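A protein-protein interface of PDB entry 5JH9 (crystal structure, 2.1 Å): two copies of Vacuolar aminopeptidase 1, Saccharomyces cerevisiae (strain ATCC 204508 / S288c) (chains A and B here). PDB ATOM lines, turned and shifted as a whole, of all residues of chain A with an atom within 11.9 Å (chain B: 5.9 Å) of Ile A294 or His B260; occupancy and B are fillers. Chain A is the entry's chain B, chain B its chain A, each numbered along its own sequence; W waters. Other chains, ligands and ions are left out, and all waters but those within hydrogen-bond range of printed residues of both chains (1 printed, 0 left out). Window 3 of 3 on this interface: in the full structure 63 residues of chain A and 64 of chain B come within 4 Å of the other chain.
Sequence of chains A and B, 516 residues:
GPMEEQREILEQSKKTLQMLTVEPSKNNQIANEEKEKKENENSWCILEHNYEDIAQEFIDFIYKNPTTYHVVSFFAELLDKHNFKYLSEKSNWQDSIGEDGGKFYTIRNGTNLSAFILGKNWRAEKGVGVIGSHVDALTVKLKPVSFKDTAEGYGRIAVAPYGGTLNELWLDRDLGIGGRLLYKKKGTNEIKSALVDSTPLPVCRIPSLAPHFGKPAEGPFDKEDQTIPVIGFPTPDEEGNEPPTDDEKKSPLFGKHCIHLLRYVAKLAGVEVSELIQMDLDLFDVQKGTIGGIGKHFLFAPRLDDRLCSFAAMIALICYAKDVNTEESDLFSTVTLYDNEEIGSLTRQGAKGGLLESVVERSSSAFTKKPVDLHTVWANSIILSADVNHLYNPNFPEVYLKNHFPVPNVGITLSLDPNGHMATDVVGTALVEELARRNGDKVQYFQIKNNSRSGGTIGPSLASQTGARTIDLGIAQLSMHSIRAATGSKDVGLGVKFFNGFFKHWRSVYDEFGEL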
ATOM      1  N   THR A 290     -11.697  20.078   3.326  1.00  0.00           N
ATOM      2  CA  THR A 290     -10.455  20.821   3.548  1.00  0.00           C
ATOM      3  C   THR A 290      -9.720  20.370   4.803  1.00  0.00           C
ATOM      4  O   THR A 290     -10.323  19.842   5.746  1.00  0.00           O
ATOM      5  CB  THR A 290     -10.713  22.348   3.604  1.00  0.00           C
ATOM      6  OG1 THR A 290      -9.467  23.050   3.721  1.00  0.00           O
ATOM      7  CG2 THR A 290     -11.601  22.718   4.765  1.00  0.00           C
ATOM      8  N   ILE A 291      -8.410  20.581   4.792  1.00  0.00           N
ATOM      9  CA  ILE A 291      -7.588  20.413   5.976  1.00  0.00           C
ATOM     10  C   ILE A 291      -7.858  21.647   6.831  1.00  0.00           C
ATOM     11  O   ILE A 291      -8.002  22.747   6.302  1.00  0.00           O
ATOM     12  CB  ILE A 291      -6.077  20.317   5.643  1.00  0.00           C
ATOM     13  CG1 ILE A 291      -5.788  19.168   4.659  1.00  0.00           C
ATOM     14  CG2 ILE A 291      -5.259  20.139   6.915  1.00  0.00           C
ATOM     15  CD1 ILE A 291      -6.235  17.797   5.124  1.00  0.00           C
ATOM     16  N   GLY A 292      -7.935  21.451   8.144  1.00  0.00           N
ATOM     17  CA  GLY A 292      -8.251  22.525   9.079  1.00  0.00           C
ATOM     18  C   GLY A 292      -7.687  22.299  10.466  1.00  0.00           C
ATOM     19  O   GLY A 292      -7.020  21.286  10.735  1.00  0.00           O
ATOM     20  N   GLY A 293      -7.999  23.239  11.350  1.00  0.00           N
ATOM     21  CA  GLY A 293      -7.369  23.337  12.654  1.00  0.00           C
ATOM     22  C   GLY A 293      -6.204  24.307  12.555  1.00  0.00           C
ATOM     23  O   GLY A 293      -5.587  24.438  11.491  1.00  0.00           O
ATOM     24  N   ILE A 294      -5.887  24.979  13.658  1.00  0.00           N
ATOM     25  CA  ILE A 294      -4.789  25.953  13.663  1.00  0.00           C
ATOM     26  C   ILE A 294      -3.420  25.318  13.363  1.00  0.00           C
ATOM     27  O   ILE A 294      -2.539  26.003  12.860  1.00  0.00           O
ATOM     28  CB  ILE A 294      -4.745  26.771  14.979  1.00  0.00           C
ATOM     29  CG1 ILE A 294      -3.937  28.063  14.792  1.00  0.00           C
ATOM     30  CG2 ILE A 294      -4.215  25.937  16.142  1.00  0.00           C
ATOM     31  CD1 ILE A 294      -4.184  29.093  15.871  1.00  0.00           C
ATOM     32  N   GLY A 295      -3.260  24.027  13.674  1.00  0.00           N
ATOM     33  CA  GLY A 295      -2.072  23.250  13.300  1.00  0.00           C
ATOM     34  C   GLY A 295      -2.312  22.214  12.209  1.00  0.00           C
ATOM     35  O   GLY A 295      -1.506  21.296  12.044  1.00  0.00           O
ATOM     36  N   LYS A 296      -3.391  22.379  11.442  1.00  0.00           N
ATOM     37  CA  LYS A 296      -3.791  21.444  10.383  1.00  0.00           C
ATOM     38  C   LYS A 296      -3.908  19.975  10.845  1.00  0.00           C
ATOM     39  O   LYS A 296      -3.566  19.053  10.106  1.00  0.00           O
ATOM     40  CB  LYS A 296      -2.877  21.606   9.160  1.00  0.00           C
ATOM     41  CG  LYS A 296      -3.030  22.975   8.510  1.00  0.00           C
ATOM     42  CD  LYS A 296      -2.212  23.119   7.237  1.00  0.00           C
ATOM     43  CE  LYS A 296      -2.408  24.498   6.634  1.00  0.00           C
ATOM     44  NZ  LYS A 296      -1.832  24.604   5.268  1.00  0.00           N
ATOM     45  N   HIS A 297      -4.413  19.778  12.063  1.00  0.00           N
ATOM     46  CA  HIS A 297      -4.602  18.437  12.639  1.00  0.00           C
ATOM     47  C   HIS A 297      -5.892  17.759  12.179  1.00  0.00           C
ATOM     48  O   HIS A 297      -6.063  16.565  12.420  1.00  0.00           O
ATOM     49  CB  HIS A 297      -4.632  18.494  14.174  1.00  0.00           C
ATOM     50  CG  HIS A 297      -3.371  19.018  14.793  1.00  0.00           C
ATOM     51  ND1 HIS A 297      -3.326  20.199  15.509  1.00  0.00           N
ATOM     52  CD2 HIS A 297      -2.115  18.513  14.820  1.00  0.00           C
ATOM     53  CE1 HIS A 297      -2.096  20.400  15.944  1.00  0.00           C
ATOM     54  NE2 HIS A 297      -1.341  19.391  15.540  1.00  0.00           N
ATOM     55  N   PHE A 298      -6.797  18.505  11.541  1.00  0.00           N
ATOM     56  CA  PHE A 298      -8.110  17.978  11.150  1.00  0.00           C
ATOM     57  C   PHE A 298      -8.330  17.961   9.647  1.00  0.00           C
ATOM     58  O   PHE A 298      -7.671  18.687   8.896  1.00  0.00           O
ATOM     59  CB  PHE A 298      -9.230  18.810  11.786  1.00  0.00           C
ATOM     60  CG  PHE A 298      -9.218  18.793  13.283  1.00  0.00           C
ATOM     61  CD1 PHE A 298      -9.408  17.602  13.973  1.00  0.00           C
ATOM     62  CD2 PHE A 298      -9.029  19.964  14.006  1.00  0.00           C
ATOM     63  CE1 PHE A 298      -9.396  17.575  15.357  1.00  0.00           C
ATOM     64  CE2 PHE A 298      -9.019  19.942  15.390  1.00  0.00           C
ATOM     65  CZ  PHE A 298      -9.200  18.747  16.066  1.00  0.00           C
ATOM     66  N   LEU A 299      -9.284  17.128   9.242  1.00  0.00           N
ATOM     67  CA  LEU A 299      -9.817  17.089   7.889  1.00  0.00           C
ATOM     68  C   LEU A 299     -11.335  17.214   7.999  1.00  0.00           C
ATOM     69  O   LEU A 299     -11.978  16.402   8.662  1.00  0.00           O
ATOM     70  CB  LEU A 299      -9.428  15.770   7.224  1.00  0.00           C
ATOM     71  CG  LEU A 299      -9.740  15.524   5.742  1.00  0.00           C
ATOM     72  CD1 LEU A 299      -8.809  14.446   5.181  1.00  0.00           C
ATOM     73  CD2 LEU A 299     -11.196  15.122   5.513  1.00  0.00           C
ATOM     74  N   PHE A 300     -11.895  18.247   7.370  1.00  0.00           N
ATOM     75  CA  PHE A 300     -13.349  18.476   7.366  1.00  0.00           C
ATOM     76  C   PHE A 300     -13.918  18.089   6.011  1.00  0.00           C
ATOM     77  O   PHE A 300     -13.449  18.575   4.997  1.00  0.00           O
ATOM     78  CB  PHE A 300     -13.673  19.954   7.641  1.00  0.00           C
ATOM     79  CG  PHE A 300     -12.994  20.526   8.862  1.00  0.00           C
ATOM     80  CD1 PHE A 300     -12.823  19.768  10.021  1.00  0.00           C
ATOM     81  CD2 PHE A 300     -12.560  21.848   8.864  1.00  0.00           C
ATOM     82  CE1 PHE A 300     -12.211  20.313  11.144  1.00  0.00           C
ATOM     83  CE2 PHE A 300     -11.956  22.398   9.986  1.00  0.00           C
ATOM     84  CZ  PHE A 300     -11.780  21.630  11.130  1.00  0.00           C
ATOM     85  N   PRO A 408      -7.725  11.935  17.699  1.00  0.00           N
ATOM     86  CA  PRO A 408      -7.258  12.055  16.314  1.00  0.00           C
ATOM     87  C   PRO A 408      -5.790  11.680  16.111  1.00  0.00           C
ATOM     88  O   PRO A 408      -4.984  11.796  17.033  1.00  0.00           O
ATOM     89  CB  PRO A 408      -7.444  13.551  16.006  1.00  0.00           C
ATOM     90  CG  PRO A 408      -8.422  14.040  17.026  1.00  0.00           C
ATOM     91  CD  PRO A 408      -8.065  13.260  18.252  1.00  0.00           C
ATOM     92  N   ASN A 409      -5.478  11.237  14.896  1.00  0.00           N
ATOM     93  CA  ASN A 409      -4.107  11.063  14.414  1.00  0.00           C
ATOM     94  C   ASN A 409      -3.262  10.056  15.202  1.00  0.00           C
ATOM     95  O   ASN A 409      -2.049  10.223  15.315  1.00  0.00           O
ATOM     96  CB  ASN A 409      -3.395  12.430  14.338  1.00  0.00           C
ATOM     97  CG  ASN A 409      -4.147  13.430  13.479  1.00  0.00           C
ATOM     98  OD1 ASN A 409      -4.610  13.093  12.386  1.00  0.00           O
ATOM     99  ND2 ASN A 409      -4.283  14.659  13.968  1.00  0.00           N
ATOM    100  N   ALA A 486     -15.829  15.562  10.630  1.00  0.00           N
ATOM    101  CA  ALA A 486     -14.387  15.769  10.810  1.00  0.00           C
ATOM    102  C   ALA A 486     -13.675  14.511  11.303  1.00  0.00           C
ATOM    103  O   ALA A 486     -14.237  13.729  12.073  1.00  0.00           O
ATOM    104  CB  ALA A 486     -14.146  16.911  11.784  1.00  0.00           C
ATOM    105  N   THR A 487     -12.439  14.325  10.832  1.00  0.00           N
ATOM    106  CA  THR A 487     -11.508  13.322  11.366  1.00  0.00           C
ATOM    107  C   THR A 487     -10.115  13.957  11.419  1.00  0.00           C
ATOM    108  O   THR A 487      -9.951  15.135  11.079  1.00  0.00           O
ATOM    109  CB  THR A 487     -11.505  12.015  10.522  1.00  0.00           C
ATOM    110  OG1 THR A 487     -10.709  11.013  11.164  1.00  0.00           O
ATOM    111  CG2 THR A 487     -10.969  12.240   9.114  1.00  0.00           C
ATOM    112  N   GLY A 488      -9.114  13.198  11.855  1.00  0.00           N
ATOM    113  CA  GLY A 488      -7.742  13.701  11.871  1.00  0.00           C
ATOM    114  C   GLY A 488      -7.163  13.767  10.464  1.00  0.00           C
ATOM    115  O   GLY A 488      -7.504  12.946   9.614  1.00  0.00           O
ATOM    116  N   SER A 489      -6.293  14.745  10.219  1.00  0.00           N
ATOM    117  CA  SER A 489      -5.643  14.904   8.914  1.00  0.00           C
ATOM    118  C   SER A 489      -4.697  13.744   8.568  1.00  0.00           C
ATOM    119  O   SER A 489      -4.493  13.470   7.393  1.00  0.00           O
ATOM    120  CB  SER A 489      -4.892  16.241   8.831  1.00  0.00           C
ATOM    121  OG  SER A 489      -3.957  16.378   9.884  1.00  0.00           O
ATOM    122  N   ILE B 177     -10.561  32.622  11.669  1.00  0.00           N
ATOM    123  CA  ILE B 177     -10.349  33.578  12.752  1.00  0.00           C
ATOM    124  C   ILE B 177      -9.766  34.859  12.162  1.00  0.00           C
ATOM    125  O   ILE B 177      -8.945  34.816  11.244  1.00  0.00           O
ATOM    126  CB  ILE B 177      -9.452  33.001  13.877  1.00  0.00           C
ATOM    127  CG1 ILE B 177      -9.393  33.966  15.072  1.00  0.00           C
ATOM    128  CG2 ILE B 177      -8.045  32.678  13.386  1.00  0.00           C
ATOM    129  CD1 ILE B 177      -8.816  33.357  16.335  1.00  0.00           C
ATOM    130  N   LEU B 201      -7.844  29.228   5.665  1.00  0.00           N
ATOM    131  CA  LEU B 201      -7.690  28.200   6.705  1.00  0.00           C
ATOM    132  C   LEU B 201      -8.800  28.289   7.751  1.00  0.00           C
ATOM    133  O   LEU B 201      -8.881  29.294   8.468  1.00  0.00           O
ATOM    134  CB  LEU B 201      -6.335  28.320   7.419  1.00  0.00           C
ATOM    135  CG  LEU B 201      -6.120  27.358   8.603  1.00  0.00           C
ATOM    136  CD1 LEU B 201      -6.048  25.922   8.105  1.00  0.00           C
ATOM    137  CD2 LEU B 201      -4.876  27.724   9.393  1.00  0.00           C
ATOM    138  N   PRO B 202      -9.648  27.240   7.860  1.00  0.00           N
ATOM    139  CA  PRO B 202     -10.545  27.221   9.011  1.00  0.00           C
ATOM    140  C   PRO B 202      -9.795  26.695  10.237  1.00  0.00           C
ATOM    141  O   PRO B 202      -9.460  25.506  10.300  1.00  0.00           O
ATOM    142  CB  PRO B 202     -11.675  26.284   8.572  1.00  0.00           C
ATOM    143  CG  PRO B 202     -11.167  25.522   7.382  1.00  0.00           C
ATOM    144  CD  PRO B 202      -9.776  26.001   7.065  1.00  0.00           C
ATOM    145  N   VAL B 203      -9.509  27.591  11.181  1.00  0.00           N
ATOM    146  CA  VAL B 203      -8.732  27.235  12.373  1.00  0.00           C
ATOM    147  C   VAL B 203      -9.519  26.406  13.391  1.00  0.00           C
ATOM    148  O   VAL B 203      -8.925  25.787  14.266  1.00  0.00           O
ATOM    149  CB  VAL B 203      -8.106  28.472  13.077  1.00  0.00           C
ATOM    150  CG1 VAL B 203      -7.161  29.187  12.128  1.00  0.00           C
ATOM    151  CG2 VAL B 203      -9.161  29.435  13.620  1.00  0.00           C
ATOM    152  N   CYS B 204     -10.846  26.402  13.293  1.00  0.00           N
ATOM    153  CA  CYS B 204     -11.650  25.665  14.249  1.00  0.00           C
ATOM    154  C   CYS B 204     -13.025  25.309  13.703  1.00  0.00           C
ATOM    155  O   CYS B 204     -13.384  25.677  12.579  1.00  0.00           O
ATOM    156  CB  CYS B 204     -11.774  26.468  15.548  1.00  0.00           C
ATOM    157  SG  CYS B 204     -12.754  27.960  15.362  1.00  0.00           S
ATOM    158  N   ILE B 231     -10.066  23.890  18.261  1.00  0.00           N
ATOM    159  CA  ILE B 231      -9.045  24.550  17.455  1.00  0.00           C
ATOM    160  C   ILE B 231      -7.893  23.612  17.048  1.00  0.00           C
ATOM    161  O   ILE B 231      -7.243  23.836  16.025  1.00  0.00           O
ATOM    162  CB  ILE B 231      -8.539  25.827  18.182  1.00  0.00           C
ATOM    163  CG1 ILE B 231      -7.988  26.843  17.177  1.00  0.00           C
ATOM    164  CG2 ILE B 231      -7.515  25.505  19.268  1.00  0.00           C
ATOM    165  CD1 ILE B 231      -7.683  28.192  17.794  1.00  0.00           C
ATOM    166  N   GLY B 232      -7.646  22.557  17.825  1.00  0.00           N
ATOM    167  CA  GLY B 232      -6.598  21.602  17.469  1.00  0.00           C
ATOM    168  C   GLY B 232      -6.500  20.379  18.349  1.00  0.00           C
ATOM    169  O   GLY B 232      -7.338  20.144  19.229  1.00  0.00           O
ATOM    170  N   PRO B 234      -2.832  19.119  19.546  1.00  0.00           N
ATOM    171  CA  PRO B 234      -1.371  19.169  19.377  1.00  0.00           C
ATOM    172  C   PRO B 234      -0.624  17.944  19.908  1.00  0.00           C
ATOM    173  O   PRO B 234      -1.042  17.337  20.895  1.00  0.00           O
ATOM    174  CB  PRO B 234      -0.964  20.429  20.150  1.00  0.00           C
ATOM    175  CG  PRO B 234      -2.050  20.648  21.138  1.00  0.00           C
ATOM    176  CD  PRO B 234      -3.310  20.121  20.518  1.00  0.00           C
ATOM    177  N   CYS B 258      -3.778  30.870  24.423  1.00  0.00           N
ATOM    178  CA  CYS B 258      -2.883  29.773  24.059  1.00  0.00           C
ATOM    179  C   CYS B 258      -1.683  30.276  23.241  1.00  0.00           C
ATOM    180  O   CYS B 258      -1.856  31.060  22.310  1.00  0.00           O
ATOM    181  CB  CYS B 258      -3.695  28.754  23.243  1.00  0.00           C
ATOM    182  SG  CYS B 258      -2.787  27.361  22.583  1.00  0.00           S
ATOM    183  N   ILE B 259      -0.474  29.844  23.600  1.00  0.00           N
ATOM    184  CA  ILE B 259       0.749  30.280  22.893  1.00  0.00           C
ATOM    185  C   ILE B 259       0.733  29.917  21.394  1.00  0.00           C
ATOM    186  O   ILE B 259       1.257  30.670  20.578  1.00  0.00           O
ATOM    187  CB  ILE B 259       2.043  29.759  23.588  1.00  0.00           C
ATOM    188  CG1 ILE B 259       3.297  30.491  23.083  1.00  0.00           C
ATOM    189  CG2 ILE B 259       2.211  28.252  23.403  1.00  0.00           C
ATOM    190  CD1 ILE B 259       3.336  31.971  23.389  1.00  0.00           C
ATOM    191  N   HIS B 260       0.112  28.792  21.035  1.00  0.00           N
ATOM    192  CA  HIS B 260      -0.066  28.432  19.620  1.00  0.00           C
ATOM    193  C   HIS B 260      -0.874  29.521  18.911  1.00  0.00           C
ATOM    194  O   HIS B 260      -0.487  29.981  17.837  1.00  0.00           O
ATOM    195  CB  HIS B 260      -0.754  27.066  19.469  1.00  0.00           C
ATOM    196  CG  HIS B 260      -0.487  26.375  18.161  1.00  0.00           C
ATOM    197  ND1 HIS B 260      -0.388  27.041  16.955  1.00  0.00           N
ATOM    198  CD2 HIS B 260      -0.335  25.060  17.870  1.00  0.00           C
ATOM    199  CE1 HIS B 260      -0.169  26.171  15.985  1.00  0.00           C
ATOM    200  NE2 HIS B 260      -0.135  24.962  16.514  1.00  0.00           N
ATOM    201  N   LEU B 261      -1.982  29.940  19.522  1.00  0.00           N
ATOM    202  CA  LEU B 261      -2.808  31.017  18.967  1.00  0.00           C
ATOM    203  C   LEU B 261      -2.049  32.346  18.861  1.00  0.00           C
ATOM    204  O   LEU B 261      -2.113  33.004  17.823  1.00  0.00           O
ATOM    205  CB  LEU B 261      -4.091  31.214  19.782  1.00  0.00           C
ATOM    206  CG  LEU B 261      -5.056  32.305  19.304  1.00  0.00           C
ATOM    207  CD1 LEU B 261      -5.417  32.135  17.834  1.00  0.00           C
ATOM    208  CD2 LEU B 261      -6.310  32.308  20.165  1.00  0.00           C
ATOM    209  N   LEU B 262      -1.332  32.723  19.921  1.00  0.00           N
ATOM    210  CA  LEU B 262      -0.571  33.983  19.934  1.00  0.00           C
ATOM    211  C   LEU B 262       0.472  34.039  18.829  1.00  0.00           C
ATOM    212  O   LEU B 262       0.582  35.050  18.125  1.00  0.00           O
ATOM    213  CB  LEU B 262       0.112  34.210  21.288  1.00  0.00           C
ATOM    214  CG  LEU B 262      -0.804  34.527  22.473  1.00  0.00           C
ATOM    215  CD1 LEU B 262      -0.001  34.637  23.758  1.00  0.00           C
ATOM    216  CD2 LEU B 262      -1.607  35.799  22.231  1.00  0.00           C
ATOM    217  N   ARG B 263       1.240  32.955  18.692  1.00  0.00           N
ATOM    218  CA  ARG B 263       2.212  32.816  17.608  1.00  0.00           C
ATOM    219  C   ARG B 263       1.558  32.948  16.235  1.00  0.00           C
ATOM    220  O   ARG B 263       2.115  33.598  15.343  1.00  0.00           O
ATOM    221  CB  ARG B 263       2.948  31.468  17.695  1.00  0.00           C
ATOM    222  CG  ARG B 263       3.963  31.403  18.822  1.00  0.00           C
ATOM    223  CD  ARG B 263       4.494  29.993  19.042  1.00  0.00           C
ATOM    224  NE  ARG B 263       5.317  29.915  20.249  1.00  0.00           N
ATOM    225  CZ  ARG B 263       5.665  28.792  20.877  1.00  0.00           C
ATOM    226  NH1 ARG B 263       6.415  28.865  21.971  1.00  0.00           N
ATOM    227  NH2 ARG B 263       5.270  27.596  20.443  1.00  0.00           N
ATOM    228  N   TYR B 264       0.386  32.330  16.071  1.00  0.00           N
ATOM    229  CA  TYR B 264      -0.299  32.307  14.781  1.00  0.00           C
ATOM    230  C   TYR B 264      -0.732  33.706  14.340  1.00  0.00           C
ATOM    231  O   TYR B 264      -0.384  34.137  13.240  1.00  0.00           O
ATOM    232  CB  TYR B 264      -1.495  31.344  14.801  1.00  0.00           C
ATOM    233  CG  TYR B 264      -2.234  31.307  13.490  1.00  0.00           C
ATOM    234  CD1 TYR B 264      -1.670  30.697  12.369  1.00  0.00           C
ATOM    235  CD2 TYR B 264      -3.488  31.907  13.355  1.00  0.00           C
ATOM    236  CE1 TYR B 264      -2.340  30.672  11.154  1.00  0.00           C
ATOM    237  CE2 TYR B 264      -4.167  31.886  12.144  1.00  0.00           C
ATOM    238  CZ  TYR B 264      -3.590  31.270  11.047  1.00  0.00           C
ATOM    239  OH  TYR B 264      -4.263  31.250   9.851  1.00  0.00           O
ATOM    240  N   VAL B 265      -1.468  34.411  15.201  1.00  0.00           N
ATOM    241  CA  VAL B 265      -1.890  35.792  14.900  1.00  0.00           C
ATOM    242  C   VAL B 265      -0.710  36.776  14.815  1.00  0.00           C
ATOM    243  O   VAL B 265      -0.769  37.738  14.050  1.00  0.00           O
ATOM    244  CB  VAL B 265      -2.989  36.324  15.864  1.00  0.00           C
ATOM    245  CG1 VAL B 265      -4.214  35.418  15.820  1.00  0.00           C
ATOM    246  CG2 VAL B 265      -2.479  36.483  17.292  1.00  0.00           C
HETATM  247  O   HOH W   1      -5.098  21.715  14.506  1.00  0.00           O
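The backbone carbonyl oxygen (O) of Pro B202 sits at hydrogen-bond distance from the backbone NH (N) of Gly A293, 2.9 Å away.
O of Ile B231 lies within hydrogen-bond range of N of Ile A294 (3.0 Å).
O of Val B203 lies within hydrogen-bond range of N of Ile A294, 3.2 Å away.
N of Phe A300 is in hydrogen-bond range of O of Thr A290 (2.8 Å).
The side-chain sulfur of Cys B258 sits close to the backbone NH of His B260, at 3.6 Å.
The side-chain amide nitrogen of Asn A409 is in hydrogen-bond range of the backbone carbonyl oxygen of His A297.
The backbone NH (N) of His A297 lies within hydrogen-bond range of the backbone carbonyl oxygen (O) of Gly A292 (3.3 Å).
The backbone carbonyl oxygen of His A297 lies within hydrogen-bond range of the backbone NH of Ser A489, at 2.9 Å.
N of Gly A292 lies within hydrogen-bond range of O of Phe A298 (2.9 Å).
Pro B202 touches Thr A290.
CD of Pro B202 touches O of Ile A291, 3.8 Å away.
Gly A293 touches Leu B201 (O to CD1, 3.7 Å).
Val B203 touches Gly A293.
O of Ile A294 touches CE1 of His B260, 3.9 Å away.
Ile A294 touches Leu B261.
CD1 of Ile A294 touches CB of Tyr B264 (3.7 Å).
Pro B234 touches His A297 (CA to CE1, 3.7 Å).
Gly B232 touches Phe A298.
CE2 of Phe A300 touches O of Pro B202, at 3.999 Å.
Of the printed residues of chain B, Ile A294 touches Val B203 (3.2 Å), Ile B231 (3.0 Å), His B260 (3.9 Å), Leu B261 (3.8 Å) and Tyr B264 (3.7 Å).
His B260 touches just one residue of chain A: Ile A294 (3.9 Å).
Of chain A, only Gly A293 and Ile A294 come within 4 Å of Ile B231.
Of chain A, only Phe A298 (3.6 Å) comes within 4 Å of Gly B232.
No residue of chain A comes within 4 Å of Ile B259.
Of chain A, only Ile A294 comes within 4 Å of Leu B261.
Printed residues of chain A within 4 Å of Pro B234: His A297 (3.7 Å).
Of the printed residues of chain B, Phe A298 touches Gly B232 (3.6 Å).
Of the printed residues of chain B, Gly A292 touches Pro B202 (3.4 Å).
Of the printed residues of chain B, His A297 touches Pro B234.
Pro A408 touches none of the printed residues of chain B.
Gly A295 touches none of the printed residues of chain B.
The nearest residue of chain A that does not touch His B260 is Gly A295 (4.1 Å).
Printed residues of chain B that touch a printed residue of chain A: Leu B201, Pro B202, Val B203, Ile B231, Gly B232, Pro B234, His B260, Leu B261 and Tyr B264.
Hydrophobic or aromatic side chains of chain B within 4 Å of the printed part of chain A: Leu B201, Pro B202, Ile B231, His B260, Leu B261 and Tyr B264.
Hydrophobic or aromatic side chains of chain A within 4 Å of the printed part of chain B: Ile A294, His A297, Phe A298 and Phe A300.
Along chain A the printed residues that touch a printed residue of chain B span positions 290 to 300.
No position is printed for both chains.
Of the 15 pairs that touch across the chains among the printed residues, none has its exchanged pair printed and touching as well.
Water W1 lies within hydrogen-bond range of ND1 of His A297 (2.5 Å), N of Gly A295 (3.1 Å), O of Ile B231 (3.4 Å) and N of Ile A294 (3.5 Å).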
